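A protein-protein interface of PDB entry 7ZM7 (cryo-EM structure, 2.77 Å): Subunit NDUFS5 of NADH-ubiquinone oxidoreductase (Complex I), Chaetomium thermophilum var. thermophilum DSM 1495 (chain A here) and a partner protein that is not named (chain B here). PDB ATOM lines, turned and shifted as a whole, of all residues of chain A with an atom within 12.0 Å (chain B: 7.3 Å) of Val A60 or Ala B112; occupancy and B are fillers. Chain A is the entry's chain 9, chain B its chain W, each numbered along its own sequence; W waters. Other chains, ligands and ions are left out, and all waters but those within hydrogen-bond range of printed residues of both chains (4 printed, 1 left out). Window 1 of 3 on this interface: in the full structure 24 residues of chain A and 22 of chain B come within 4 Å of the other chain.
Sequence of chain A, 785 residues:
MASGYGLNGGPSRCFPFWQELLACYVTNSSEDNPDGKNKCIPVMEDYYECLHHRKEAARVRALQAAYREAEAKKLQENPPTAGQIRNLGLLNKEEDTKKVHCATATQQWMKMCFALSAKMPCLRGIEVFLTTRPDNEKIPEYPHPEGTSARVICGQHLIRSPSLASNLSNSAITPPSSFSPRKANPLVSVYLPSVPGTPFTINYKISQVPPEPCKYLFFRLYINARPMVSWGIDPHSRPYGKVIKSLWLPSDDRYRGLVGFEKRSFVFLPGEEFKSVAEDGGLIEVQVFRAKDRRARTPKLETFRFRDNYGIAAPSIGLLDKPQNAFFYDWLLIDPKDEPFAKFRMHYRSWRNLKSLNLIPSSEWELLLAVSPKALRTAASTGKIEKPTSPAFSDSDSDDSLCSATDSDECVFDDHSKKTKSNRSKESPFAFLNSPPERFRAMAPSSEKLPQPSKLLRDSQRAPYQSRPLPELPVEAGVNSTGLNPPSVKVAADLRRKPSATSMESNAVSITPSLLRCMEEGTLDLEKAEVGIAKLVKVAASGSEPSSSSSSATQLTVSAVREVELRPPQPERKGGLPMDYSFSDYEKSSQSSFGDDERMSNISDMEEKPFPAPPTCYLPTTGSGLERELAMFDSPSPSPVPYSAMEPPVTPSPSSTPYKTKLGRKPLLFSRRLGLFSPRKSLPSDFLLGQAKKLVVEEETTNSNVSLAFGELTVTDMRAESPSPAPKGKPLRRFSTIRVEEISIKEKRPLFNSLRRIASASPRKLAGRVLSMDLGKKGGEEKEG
The guanidinium group of Arg A59 is in salt-bridge range of the side-chain carboxylate of Asp B86, 2.7 Å away. The guanidinium group of Arg A59 lies within salt-bridge range of the side-chain carboxylate of Glu B90, 3.2 Å away. The backbone NH (N) of Thr B110 lies close to the side-chain carboxylate (OE1) of Glu A56, at 3.2 Å. The backbone NH of Phe B111 lies within hydrogen-bond range of the side-chain carboxylate of Glu A56. The side-chain hydroxyl (OG1) of Thr B114 lies within hydrogen-bond range of the side-chain amide nitrogen (NE2) of Gln A64 (3.2 Å). O of Thr B114 is in hydrogen-bond range of NE of Arg A68, 2.9 Å away. The backbone carbonyl oxygen of Pro B115 sits at hydrogen-bond distance from the guanidinium group of Arg A68, 3.1 Å away.
The side-chain carboxylate of Glu A49 sits at hydrogen-bond distance from the backbone NH of Arg A54, at 3.3 Å. The side-chain carboxylate (OE1) of Glu A49 sits at hydrogen-bond distance from the backbone NH (N) of Lys A55. N of Glu A56 lies within hydrogen-bond range of OE2 of Glu A49 (2.9 Å). O of Ala A57 lies close to NH1 of Arg A61 (3.5 Å). The guanidinium group (NH1) of Arg A68 sits close to the side-chain amide nitrogen (NE2) of Gln A64, 3.2 Å away.
Val B100 touches Glu A49 (CG1 to OE2, 3.2 Å). Thr B110 touches His A53. CE2 of Phe B111 touches O of His A53 (3.7 Å). Val B100 touches Lys A55. Glu A56 touches Val B100. Ala A57 touches Phe B111. Ala B112 touches Val A60. Leu A63 touches Val B113 (CD2 to CG2, 3.3 Å). Val B113 touches Gln A64 (CG2 to N, 3.6 Å). Thr B114 touches Tyr A67 (O to CE1, 3.97 Å).
Printed residues of chain B within 4 Å of Glu A56: Val B100, Thr B110 and Phe B111. Ala A58 touches none of the printed residues of chain B. Of chain B, only Ala B112 and Val B113 come within 4 Å of Val A60. Printed residues of chain B within 4 Å of Leu A63: Glu B90 and Val B113. Phe B111 touches three residues of chain A. Of the printed residues of chain A, Ala B112 touches Val A60 (3.6 Å). The nearest printed residue of chain B that does not touch Ala A57 is Val B100 (6.0 Å).
Of the 19 printed residues of chain A, 11 touch a printed residue of chain B. Hydrophobic or aromatic side chains of chain A within 4 Å of the printed part of chain B: His A53, Ala A57, Val A60, Leu A63 and Tyr A67. Along chain A the printed residues that touch a printed residue of chain B span positions 49 to 68. Of the 11 printed residues of chain B, 9 touch a printed residue of chain A. Among the printed residues, 21 pairs touch across the chains. Among the printed residues, Asp or Glu carboxylates within 4 Å of a Lys or Arg side-chain nitrogen of the other chain: Arg A59 with Asp B86 (2.7 Å) and Arg A59 with Glu B90 (3.2 Å).
Water W4 lies within hydrogen-bond range of the backbone carbonyl oxygen of Ala B112 (2.5 Å), the side-chain amide nitrogen of Gln A64 (2.6 Å) and the side-chain hydroxyl of Thr B114 (3.4 Å). Water W1 bridges OE1 of Glu A56 (2.8 Å) and N of Thr B110 (3.2 Å). Water W2 lies within hydrogen-bond range of a ring nitrogen (NE2) of His A53 (2.8 Å) and the side-chain hydroxyl (OG1) of Thr B110 (3.2 Å). Water W3 bridges the side-chain carboxylate of Glu A56 and the backbone carbonyl oxygen of Phe B111.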
ATOM      1  N   GLU A  49     -31.417  18.526 -14.637  1.00  0.00           N
ATOM      2  CA  GLU A  49     -30.695  18.356 -15.924  1.00  0.00           C
ATOM      3  C   GLU A  49     -31.618  18.631 -17.103  1.00  0.00           C
ATOM      4  O   GLU A  49     -31.216  19.371 -18.004  1.00  0.00           O
ATOM      5  CB  GLU A  49     -30.076  16.962 -15.979  1.00  0.00           C
ATOM      6  CG  GLU A  49     -29.406  16.625 -17.294  1.00  0.00           C
ATOM      7  CD  GLU A  49     -28.254  17.519 -17.708  1.00  0.00           C
ATOM      8  OE1 GLU A  49     -27.782  18.303 -16.880  1.00  0.00           O
ATOM      9  OE2 GLU A  49     -27.837  17.430 -18.863  1.00  0.00           O
ATOM     10  N   HIS A  52     -32.200  22.436 -17.425  1.00  0.00           N
ATOM     11  CA  HIS A  52     -31.016  23.274 -17.762  1.00  0.00           C
ATOM     12  C   HIS A  52     -30.032  22.679 -18.772  1.00  0.00           C
ATOM     13  O   HIS A  52     -29.504  23.480 -19.552  1.00  0.00           O
ATOM     14  CB  HIS A  52     -30.374  23.760 -16.477  1.00  0.00           C
ATOM     15  CG  HIS A  52     -31.353  24.328 -15.510  1.00  0.00           C
ATOM     16  ND1 HIS A  52     -32.107  25.446 -15.797  1.00  0.00           N
ATOM     17  CD2 HIS A  52     -31.705  23.941 -14.268  1.00  0.00           C
ATOM     18  CE1 HIS A  52     -32.888  25.717 -14.777  1.00  0.00           C
ATOM     19  NE2 HIS A  52     -32.655  24.813 -13.826  1.00  0.00           N
ATOM     20  N   HIS A  53     -29.771  21.373 -18.757  1.00  0.00           N
ATOM     21  CA  HIS A  53     -28.877  20.691 -19.739  1.00  0.00           C
ATOM     22  C   HIS A  53     -27.424  21.072 -19.522  1.00  0.00           C
ATOM     23  O   HIS A  53     -26.714  21.183 -20.507  1.00  0.00           O
ATOM     24  CB  HIS A  53     -29.241  20.955 -21.199  1.00  0.00           C
ATOM     25  CG  HIS A  53     -30.686  20.791 -21.507  1.00  0.00           C
ATOM     26  ND1 HIS A  53     -31.505  21.868 -21.746  1.00  0.00           N
ATOM     27  CD2 HIS A  53     -31.451  19.690 -21.614  1.00  0.00           C
ATOM     28  CE1 HIS A  53     -32.719  21.437 -21.972  1.00  0.00           C
ATOM     29  NE2 HIS A  53     -32.712  20.107 -21.902  1.00  0.00           N
ATOM     30  N   ARG A  54     -27.007  21.244 -18.272  1.00  0.00           N
ATOM     31  CA  ARG A  54     -25.578  21.517 -17.989  1.00  0.00           C
ATOM     32  C   ARG A  54     -24.699  20.282 -18.204  1.00  0.00           C
ATOM     33  O   ARG A  54     -23.718  20.408 -18.919  1.00  0.00           O
ATOM     34  CB  ARG A  54     -25.420  21.998 -16.549  1.00  0.00           C
ATOM     35  CG  ARG A  54     -25.981  23.383 -16.277  1.00  0.00           C
ATOM     36  CD  ARG A  54     -25.731  23.814 -14.848  1.00  0.00           C
ATOM     37  NE  ARG A  54     -24.366  23.526 -14.442  1.00  0.00           N
ATOM     38  CZ  ARG A  54     -23.365  24.399 -14.478  1.00  0.00           C
ATOM     39  NH1 ARG A  54     -22.156  24.036 -14.086  1.00  0.00           N
ATOM     40  NH2 ARG A  54     -23.577  25.633 -14.898  1.00  0.00           N
ATOM     41  N   LYS A  55     -25.058  19.109 -17.692  1.00  0.00           N
ATOM     42  CA  LYS A  55     -24.147  17.934 -17.779  1.00  0.00           C
ATOM     43  C   LYS A  55     -24.050  17.452 -19.232  1.00  0.00           C
ATOM     44  O   LYS A  55     -22.963  17.054 -19.632  1.00  0.00           O
ATOM     45  CB  LYS A  55     -24.560  16.849 -16.778  1.00  0.00           C
ATOM     46  CG  LYS A  55     -25.065  17.348 -15.436  1.00  0.00           C
ATOM     47  CD  LYS A  55     -25.815  16.289 -14.667  1.00  0.00           C
ATOM     48  CE  LYS A  55     -25.025  15.008 -14.511  1.00  0.00           C
ATOM     49  NZ  LYS A  55     -25.775  14.001 -13.728  1.00  0.00           N
ATOM     50  N   GLU A  56     -25.154  17.468 -19.980  1.00  0.00           N
ATOM     51  CA  GLU A  56     -25.139  17.120 -21.423  1.00  0.00           C
ATOM     52  C   GLU A  56     -24.296  18.119 -22.196  1.00  0.00           C
ATOM     53  O   GLU A  56     -23.595  17.711 -23.118  1.00  0.00           O
ATOM     54  CB  GLU A  56     -26.538  17.236 -21.995  1.00  0.00           C
ATOM     55  CG  GLU A  56     -26.796  16.272 -23.128  1.00  0.00           C
ATOM     56  CD  GLU A  56     -27.740  16.849 -24.162  1.00  0.00           C
ATOM     57  OE1 GLU A  56     -28.947  16.593 -24.060  1.00  0.00           O
ATOM     58  OE2 GLU A  56     -27.257  17.549 -25.063  1.00  0.00           O
ATOM     59  N   ALA A  57     -24.363  19.382 -21.817  1.00  0.00           N
ATOM     60  CA  ALA A  57     -23.581  20.432 -22.482  1.00  0.00           C
ATOM     61  C   ALA A  57     -22.119  20.153 -22.194  1.00  0.00           C
ATOM     62  O   ALA A  57     -21.310  20.282 -23.106  1.00  0.00           O
ATOM     63  CB  ALA A  57     -23.994  21.768 -21.952  1.00  0.00           C
ATOM     64  N   ALA A  58     -21.819  19.775 -20.951  1.00  0.00           N
ATOM     65  CA  ALA A  58     -20.440  19.436 -20.623  1.00  0.00           C
ATOM     66  C   ALA A  58     -19.972  18.217 -21.390  1.00  0.00           C
ATOM     67  O   ALA A  58     -18.847  18.188 -21.895  1.00  0.00           O
ATOM     68  CB  ALA A  58     -20.310  19.195 -19.125  1.00  0.00           C
ATOM     69  N   ARG A  59     -20.818  17.197 -21.490  1.00  0.00           N
ATOM     70  CA  ARG A  59     -20.438  15.994 -22.213  1.00  0.00           C
ATOM     71  C   ARG A  59     -20.227  16.259 -23.693  1.00  0.00           C
ATOM     72  O   ARG A  59     -19.199  15.864 -24.245  1.00  0.00           O
ATOM     73  CB  ARG A  59     -21.494  14.918 -22.021  1.00  0.00           C
ATOM     74  CG  ARG A  59     -21.212  13.671 -22.796  1.00  0.00           C
ATOM     75  CD  ARG A  59     -22.326  12.696 -22.643  1.00  0.00           C
ATOM     76  NE  ARG A  59     -22.368  11.765 -23.753  1.00  0.00           N
ATOM     77  CZ  ARG A  59     -22.941  12.031 -24.916  1.00  0.00           C
ATOM     78  NH1 ARG A  59     -23.512  13.207 -25.113  1.00  0.00           N
ATOM     79  NH2 ARG A  59     -22.932  11.123 -25.882  1.00  0.00           N
ATOM     80  N   VAL A  60     -21.169  16.940 -24.352  1.00  0.00           N
ATOM     81  CA  VAL A  60     -21.050  17.214 -25.779  1.00  0.00           C
ATOM     82  C   VAL A  60     -20.025  18.298 -26.073  1.00  0.00           C
ATOM     83  O   VAL A  60     -19.754  18.584 -27.243  1.00  0.00           O
ATOM     84  CB  VAL A  60     -22.442  17.551 -26.377  1.00  0.00           C
ATOM     85  CG1 VAL A  60     -22.427  17.568 -27.879  1.00  0.00           C
ATOM     86  CG2 VAL A  60     -23.456  16.514 -25.959  1.00  0.00           C
ATOM     87  N   ARG A  61     -19.420  18.892 -25.060  1.00  0.00           N
ATOM     88  CA  ARG A  61     -18.407  19.908 -25.302  1.00  0.00           C
ATOM     89  C   ARG A  61     -16.997  19.351 -25.247  1.00  0.00           C
ATOM     90  O   ARG A  61     -16.072  19.980 -25.763  1.00  0.00           O
ATOM     91  CB  ARG A  61     -18.560  21.055 -24.299  1.00  0.00           C
ATOM     92  CG  ARG A  61     -18.065  22.371 -24.796  1.00  0.00           C
ATOM     93  CD  ARG A  61     -18.130  23.437 -23.734  1.00  0.00           C
ATOM     94  NE  ARG A  61     -19.410  24.137 -23.709  1.00  0.00           N
ATOM     95  CZ  ARG A  61     -20.306  24.026 -22.733  1.00  0.00           C
ATOM     96  NH1 ARG A  61     -20.083  23.227 -21.700  1.00  0.00           N
ATOM     97  NH2 ARG A  61     -21.435  24.711 -22.794  1.00  0.00           N
ATOM     98  N   ALA A  62     -16.816  18.187 -24.625  1.00  0.00           N
ATOM     99  CA  ALA A  62     -15.559  17.458 -24.709  1.00  0.00           C
ATOM    100  C   ALA A  62     -15.552  16.505 -25.894  1.00  0.00           C
ATOM    101  O   ALA A  62     -14.542  16.374 -26.587  1.00  0.00           O
ATOM    102  CB  ALA A  62     -15.321  16.687 -23.423  1.00  0.00           C
ATOM    103  N   LEU A  63     -16.674  15.832 -26.138  1.00  0.00           N
ATOM    104  CA  LEU A  63     -16.749  14.876 -27.230  1.00  0.00           C
ATOM    105  C   LEU A  63     -16.568  15.596 -28.556  1.00  0.00           C
ATOM    106  O   LEU A  63     -16.014  15.045 -29.514  1.00  0.00           O
ATOM    107  CB  LEU A  63     -18.098  14.166 -27.198  1.00  0.00           C
ATOM    108  CG  LEU A  63     -18.371  12.925 -28.061  1.00  0.00           C
ATOM    109  CD1 LEU A  63     -19.486  12.120 -27.428  1.00  0.00           C
ATOM    110  CD2 LEU A  63     -18.636  13.137 -29.521  1.00  0.00           C
ATOM    111  N   GLN A  64     -17.064  16.828 -28.633  1.00  0.00           N
ATOM    112  CA  GLN A  64     -16.910  17.622 -29.839  1.00  0.00           C
ATOM    113  C   GLN A  64     -15.499  18.155 -29.977  1.00  0.00           C
ATOM    114  O   GLN A  64     -15.061  18.460 -31.087  1.00  0.00           O
ATOM    115  CB  GLN A  64     -17.915  18.764 -29.836  1.00  0.00           C
ATOM    116  CG  GLN A  64     -18.175  19.368 -31.190  1.00  0.00           C
ATOM    117  CD  GLN A  64     -18.695  20.768 -31.080  1.00  0.00           C
ATOM    118  OE1 GLN A  64     -18.158  21.575 -30.344  1.00  0.00           O
ATOM    119  NE2 GLN A  64     -19.752  21.063 -31.807  1.00  0.00           N
ATOM    120  N   ALA A  65     -14.785  18.299 -28.866  1.00  0.00           N
ATOM    121  CA  ALA A  65     -13.399  18.724 -28.933  1.00  0.00           C
ATOM    122  C   ALA A  65     -12.474  17.571 -29.275  1.00  0.00           C
ATOM    123  O   ALA A  65     -11.420  17.789 -29.874  1.00  0.00           O
ATOM    124  CB  ALA A  65     -12.987  19.373 -27.616  1.00  0.00           C
ATOM    125  N   ALA A  66     -12.886  16.347 -28.981  1.00  0.00           N
ATOM    126  CA  ALA A  66     -12.090  15.167 -29.359  1.00  0.00           C
ATOM    127  C   ALA A  66     -12.222  14.942 -30.853  1.00  0.00           C
ATOM    128  O   ALA A  66     -11.189  14.827 -31.523  1.00  0.00           O
ATOM    129  CB  ALA A  66     -12.612  13.968 -28.636  1.00  0.00           C
ATOM    130  N   TYR A  67     -13.454  14.874 -31.340  1.00  0.00           N
ATOM    131  CA  TYR A  67     -13.740  14.578 -32.761  1.00  0.00           C
ATOM    132  C   TYR A  67     -13.191  15.671 -33.664  1.00  0.00           C
ATOM    133  O   TYR A  67     -12.738  15.365 -34.756  1.00  0.00           O
ATOM    134  CB  TYR A  67     -15.237  14.298 -32.906  1.00  0.00           C
ATOM    135  CG  TYR A  67     -15.843  14.374 -34.283  1.00  0.00           C
ATOM    136  CD1 TYR A  67     -16.243  15.584 -34.823  1.00  0.00           C
ATOM    137  CD2 TYR A  67     -16.080  13.226 -35.017  1.00  0.00           C
ATOM    138  CE1 TYR A  67     -16.809  15.662 -36.082  1.00  0.00           C
ATOM    139  CE2 TYR A  67     -16.651  13.285 -36.275  1.00  0.00           C
ATOM    140  CZ  TYR A  67     -17.014  14.506 -36.810  1.00  0.00           C
ATOM    141  OH  TYR A  67     -17.578  14.571 -38.045  1.00  0.00           O
ATOM    142  N   ARG A  68     -13.221  16.913 -33.223  1.00  0.00           N
ATOM    143  CA  ARG A  68     -12.842  17.967 -34.184  1.00  0.00           C
ATOM    144  C   ARG A  68     -11.331  17.944 -34.425  1.00  0.00           C
ATOM    145  O   ARG A  68     -10.940  18.285 -35.543  1.00  0.00           O
ATOM    146  CB  ARG A  68     -13.424  19.319 -33.759  1.00  0.00           C
ATOM    147  CG  ARG A  68     -14.848  19.568 -34.229  1.00  0.00           C
ATOM    148  CD  ARG A  68     -15.325  20.925 -33.755  1.00  0.00           C
ATOM    149  NE  ARG A  68     -16.699  21.211 -34.132  1.00  0.00           N
ATOM    150  CZ  ARG A  68     -17.278  22.393 -33.993  1.00  0.00           C
ATOM    151  NH1 ARG A  68     -18.536  22.564 -34.360  1.00  0.00           N
ATOM    152  NH2 ARG A  68     -16.597  23.404 -33.493  1.00  0.00           N
ATOM    153  N   GLU A  69     -10.533  17.558 -33.431  1.00  0.00           N
ATOM    154  CA  GLU A  69      -9.105  17.379 -33.650  1.00  0.00           C
ATOM    155  C   GLU A  69      -8.730  15.931 -33.929  1.00  0.00           C
ATOM    156  O   GLU A  69      -7.554  15.649 -34.165  1.00  0.00           O
ATOM    157  CB  GLU A  69      -8.305  17.914 -32.456  1.00  0.00           C
ATOM    158  CG  GLU A  69      -8.629  17.269 -31.127  1.00  0.00           C
ATOM    159  CD  GLU A  69      -7.683  16.148 -30.771  1.00  0.00           C
ATOM    160  OE1 GLU A  69      -6.536  16.157 -31.266  1.00  0.00           O
ATOM    161  OE2 GLU A  69      -8.088  15.254 -29.998  1.00  0.00           O
ATOM    162  N   ARG B  82     -29.050   6.974 -34.492  1.00  0.00           N
ATOM    163  CA  ARG B  82     -28.138   8.060 -34.167  1.00  0.00           C
ATOM    164  C   ARG B  82     -27.704   8.017 -32.716  1.00  0.00           C
ATOM    165  O   ARG B  82     -26.621   8.505 -32.389  1.00  0.00           O
ATOM    166  CB  ARG B  82     -28.777   9.401 -34.496  1.00  0.00           C
ATOM    167  CG  ARG B  82     -29.148   9.538 -35.946  1.00  0.00           C
ATOM    168  CD  ARG B  82     -29.592  10.920 -36.273  1.00  0.00           C
ATOM    169  NE  ARG B  82     -28.542  11.903 -36.077  1.00  0.00           N
ATOM    170  CZ  ARG B  82     -28.302  12.886 -36.923  1.00  0.00           C
ATOM    171  NH1 ARG B  82     -27.334  13.743 -36.689  1.00  0.00           N
ATOM    172  NH2 ARG B  82     -29.038  13.001 -38.007  1.00  0.00           N
ATOM    173  N   ASP B  86     -23.682   7.595 -31.810  1.00  0.00           N
ATOM    174  CA  ASP B  86     -23.016   8.595 -30.928  1.00  0.00           C
ATOM    175  C   ASP B  86     -22.362   7.909 -29.718  1.00  0.00           C
ATOM    176  O   ASP B  86     -21.292   8.354 -29.305  1.00  0.00           O
ATOM    177  CB  ASP B  86     -23.927   9.791 -30.651  1.00  0.00           C
ATOM    178  CG  ASP B  86     -23.360  10.774 -29.644  1.00  0.00           C
ATOM    179  OD1 ASP B  86     -23.586  10.567 -28.437  1.00  0.00           O
ATOM    180  OD2 ASP B  86     -22.700  11.743 -30.076  1.00  0.00           O
ATOM    181  N   GLU B  90     -18.340   8.138 -29.155  1.00  0.00           N
ATOM    182  CA  GLU B  90     -17.731   8.512 -27.851  1.00  0.00           C
ATOM    183  C   GLU B  90     -16.782   7.440 -27.320  1.00  0.00           C
ATOM    184  O   GLU B  90     -15.700   7.793 -26.842  1.00  0.00           O
ATOM    185  CB  GLU B  90     -18.821   8.644 -26.796  1.00  0.00           C
ATOM    186  CG  GLU B  90     -18.380   9.352 -25.534  1.00  0.00           C
ATOM    187  CD  GLU B  90     -19.534   9.734 -24.624  1.00  0.00           C
ATOM    188  OE1 GLU B  90     -20.617   9.136 -24.760  1.00  0.00           O
ATOM    189  OE2 GLU B  90     -19.351  10.639 -23.794  1.00  0.00           O
ATOM    190  N   VAL B 100     -25.343  11.192 -18.607  1.00  0.00           N
ATOM    191  CA  VAL B 100     -25.893  12.562 -18.398  1.00  0.00           C
ATOM    192  C   VAL B 100     -27.135  12.486 -17.515  1.00  0.00           C
ATOM    193  O   VAL B 100     -27.440  13.492 -16.859  1.00  0.00           O
ATOM    194  CB  VAL B 100     -26.182  13.185 -19.773  1.00  0.00           C
ATOM    195  CG1 VAL B 100     -27.015  14.447 -19.684  1.00  0.00           C
ATOM    196  CG2 VAL B 100     -24.908  13.432 -20.549  1.00  0.00           C
ATOM    197  N   PRO B 109     -31.693  14.068 -27.778  1.00  0.00           N
ATOM    198  CA  PRO B 109     -30.561  14.996 -27.583  1.00  0.00           C
ATOM    199  C   PRO B 109     -30.835  16.497 -27.759  1.00  0.00           C
ATOM    200  O   PRO B 109     -31.592  16.825 -28.608  1.00  0.00           O
ATOM    201  CB  PRO B 109     -29.559  14.461 -28.602  1.00  0.00           C
ATOM    202  CG  PRO B 109     -30.363  13.694 -29.608  1.00  0.00           C
ATOM    203  CD  PRO B 109     -31.433  13.039 -28.777  1.00  0.00           C
ATOM    204  N   THR B 110     -30.273  17.372 -26.921  1.00  0.00           N
ATOM    205  CA  THR B 110     -30.478  18.791 -27.155  1.00  0.00           C
ATOM    206  C   THR B 110     -29.287  19.438 -27.824  1.00  0.00           C
ATOM    207  O   THR B 110     -29.454  20.414 -28.556  1.00  0.00           O
ATOM    208  CB  THR B 110     -30.812  19.527 -25.846  1.00  0.00           C
ATOM    209  OG1 THR B 110     -31.163  20.878 -26.133  1.00  0.00           O
ATOM    210  CG2 THR B 110     -29.669  19.549 -24.916  1.00  0.00           C
ATOM    211  N   PHE B 111     -28.104  18.882 -27.607  1.00  0.00           N
ATOM    212  CA  PHE B 111     -26.865  19.290 -28.240  1.00  0.00           C
ATOM    213  C   PHE B 111     -26.317  18.136 -29.067  1.00  0.00           C
ATOM    214  O   PHE B 111     -26.500  16.963 -28.739  1.00  0.00           O
ATOM    215  CB  PHE B 111     -25.838  19.707 -27.203  1.00  0.00           C
ATOM    216  CG  PHE B 111     -26.260  20.846 -26.348  1.00  0.00           C
ATOM    217  CD1 PHE B 111     -26.399  22.112 -26.875  1.00  0.00           C
ATOM    218  CD2 PHE B 111     -26.445  20.670 -24.991  1.00  0.00           C
ATOM    219  CE1 PHE B 111     -26.747  23.164 -26.068  1.00  0.00           C
ATOM    220  CE2 PHE B 111     -26.813  21.710 -24.193  1.00  0.00           C
ATOM    221  CZ  PHE B 111     -26.963  22.957 -24.728  1.00  0.00           C
ATOM    222  N   ALA B 112     -25.636  18.486 -30.148  1.00  0.00           N
ATOM    223  CA  ALA B 112     -25.002  17.504 -31.011  1.00  0.00           C
ATOM    224  C   ALA B 112     -23.551  17.890 -31.241  1.00  0.00           C
ATOM    225  O   ALA B 112     -23.184  19.063 -31.197  1.00  0.00           O
ATOM    226  CB  ALA B 112     -25.720  17.374 -32.360  1.00  0.00           C
ATOM    227  N   VAL B 113     -22.734  16.890 -31.457  1.00  0.00           N
ATOM    228  CA  VAL B 113     -21.380  17.107 -31.940  1.00  0.00           C
ATOM    229  C   VAL B 113     -21.437  17.308 -33.440  1.00  0.00           C
ATOM    230  O   VAL B 113     -22.047  16.521 -34.167  1.00  0.00           O
ATOM    231  CB  VAL B 113     -20.480  15.927 -31.547  1.00  0.00           C
ATOM    232  CG1 VAL B 113     -19.161  16.006 -32.217  1.00  0.00           C
ATOM    233  CG2 VAL B 113     -20.287  15.953 -30.075  1.00  0.00           C
ATOM    234  N   THR B 114     -20.829  18.385 -33.905  1.00  0.00           N
ATOM    235  CA  THR B 114     -20.879  18.748 -35.303  1.00  0.00           C
ATOM    236  C   THR B 114     -19.460  18.886 -35.813  1.00  0.00           C
ATOM    237  O   THR B 114     -18.529  19.084 -35.024  1.00  0.00           O
ATOM    238  CB  THR B 114     -21.643  20.061 -35.549  1.00  0.00           C
ATOM    239  OG1 THR B 114     -21.270  21.026 -34.573  1.00  0.00           O
ATOM    240  CG2 THR B 114     -23.128  19.852 -35.497  1.00  0.00           C
ATOM    241  N   PRO B 115     -19.260  18.768 -37.124  1.00  0.00           N
ATOM    242  CA  PRO B 115     -17.985  19.174 -37.708  1.00  0.00           C
ATOM    243  C   PRO B 115     -17.738  20.656 -37.506  1.00  0.00           C
ATOM    244  O   PRO B 115     -18.652  21.455 -37.304  1.00  0.00           O
ATOM    245  CB  PRO B 115     -18.139  18.843 -39.189  1.00  0.00           C
ATOM    246  CG  PRO B 115     -19.318  17.973 -39.281  1.00  0.00           C
ATOM    247  CD  PRO B 115     -20.175  18.198 -38.114  1.00  0.00           C
HETATM  248  O   HOH W   1     -31.683  16.090 -24.295  1.00  0.00           O
HETATM  249  O   HOH W   2     -33.679  19.659 -24.528  1.00  0.00           O
HETATM  250  O   HOH W   3     -27.042  14.618 -26.325  1.00  0.00           O
HETATM  251  O   HOH W   4     -22.328  21.361 -31.401  1.00  0.00           O
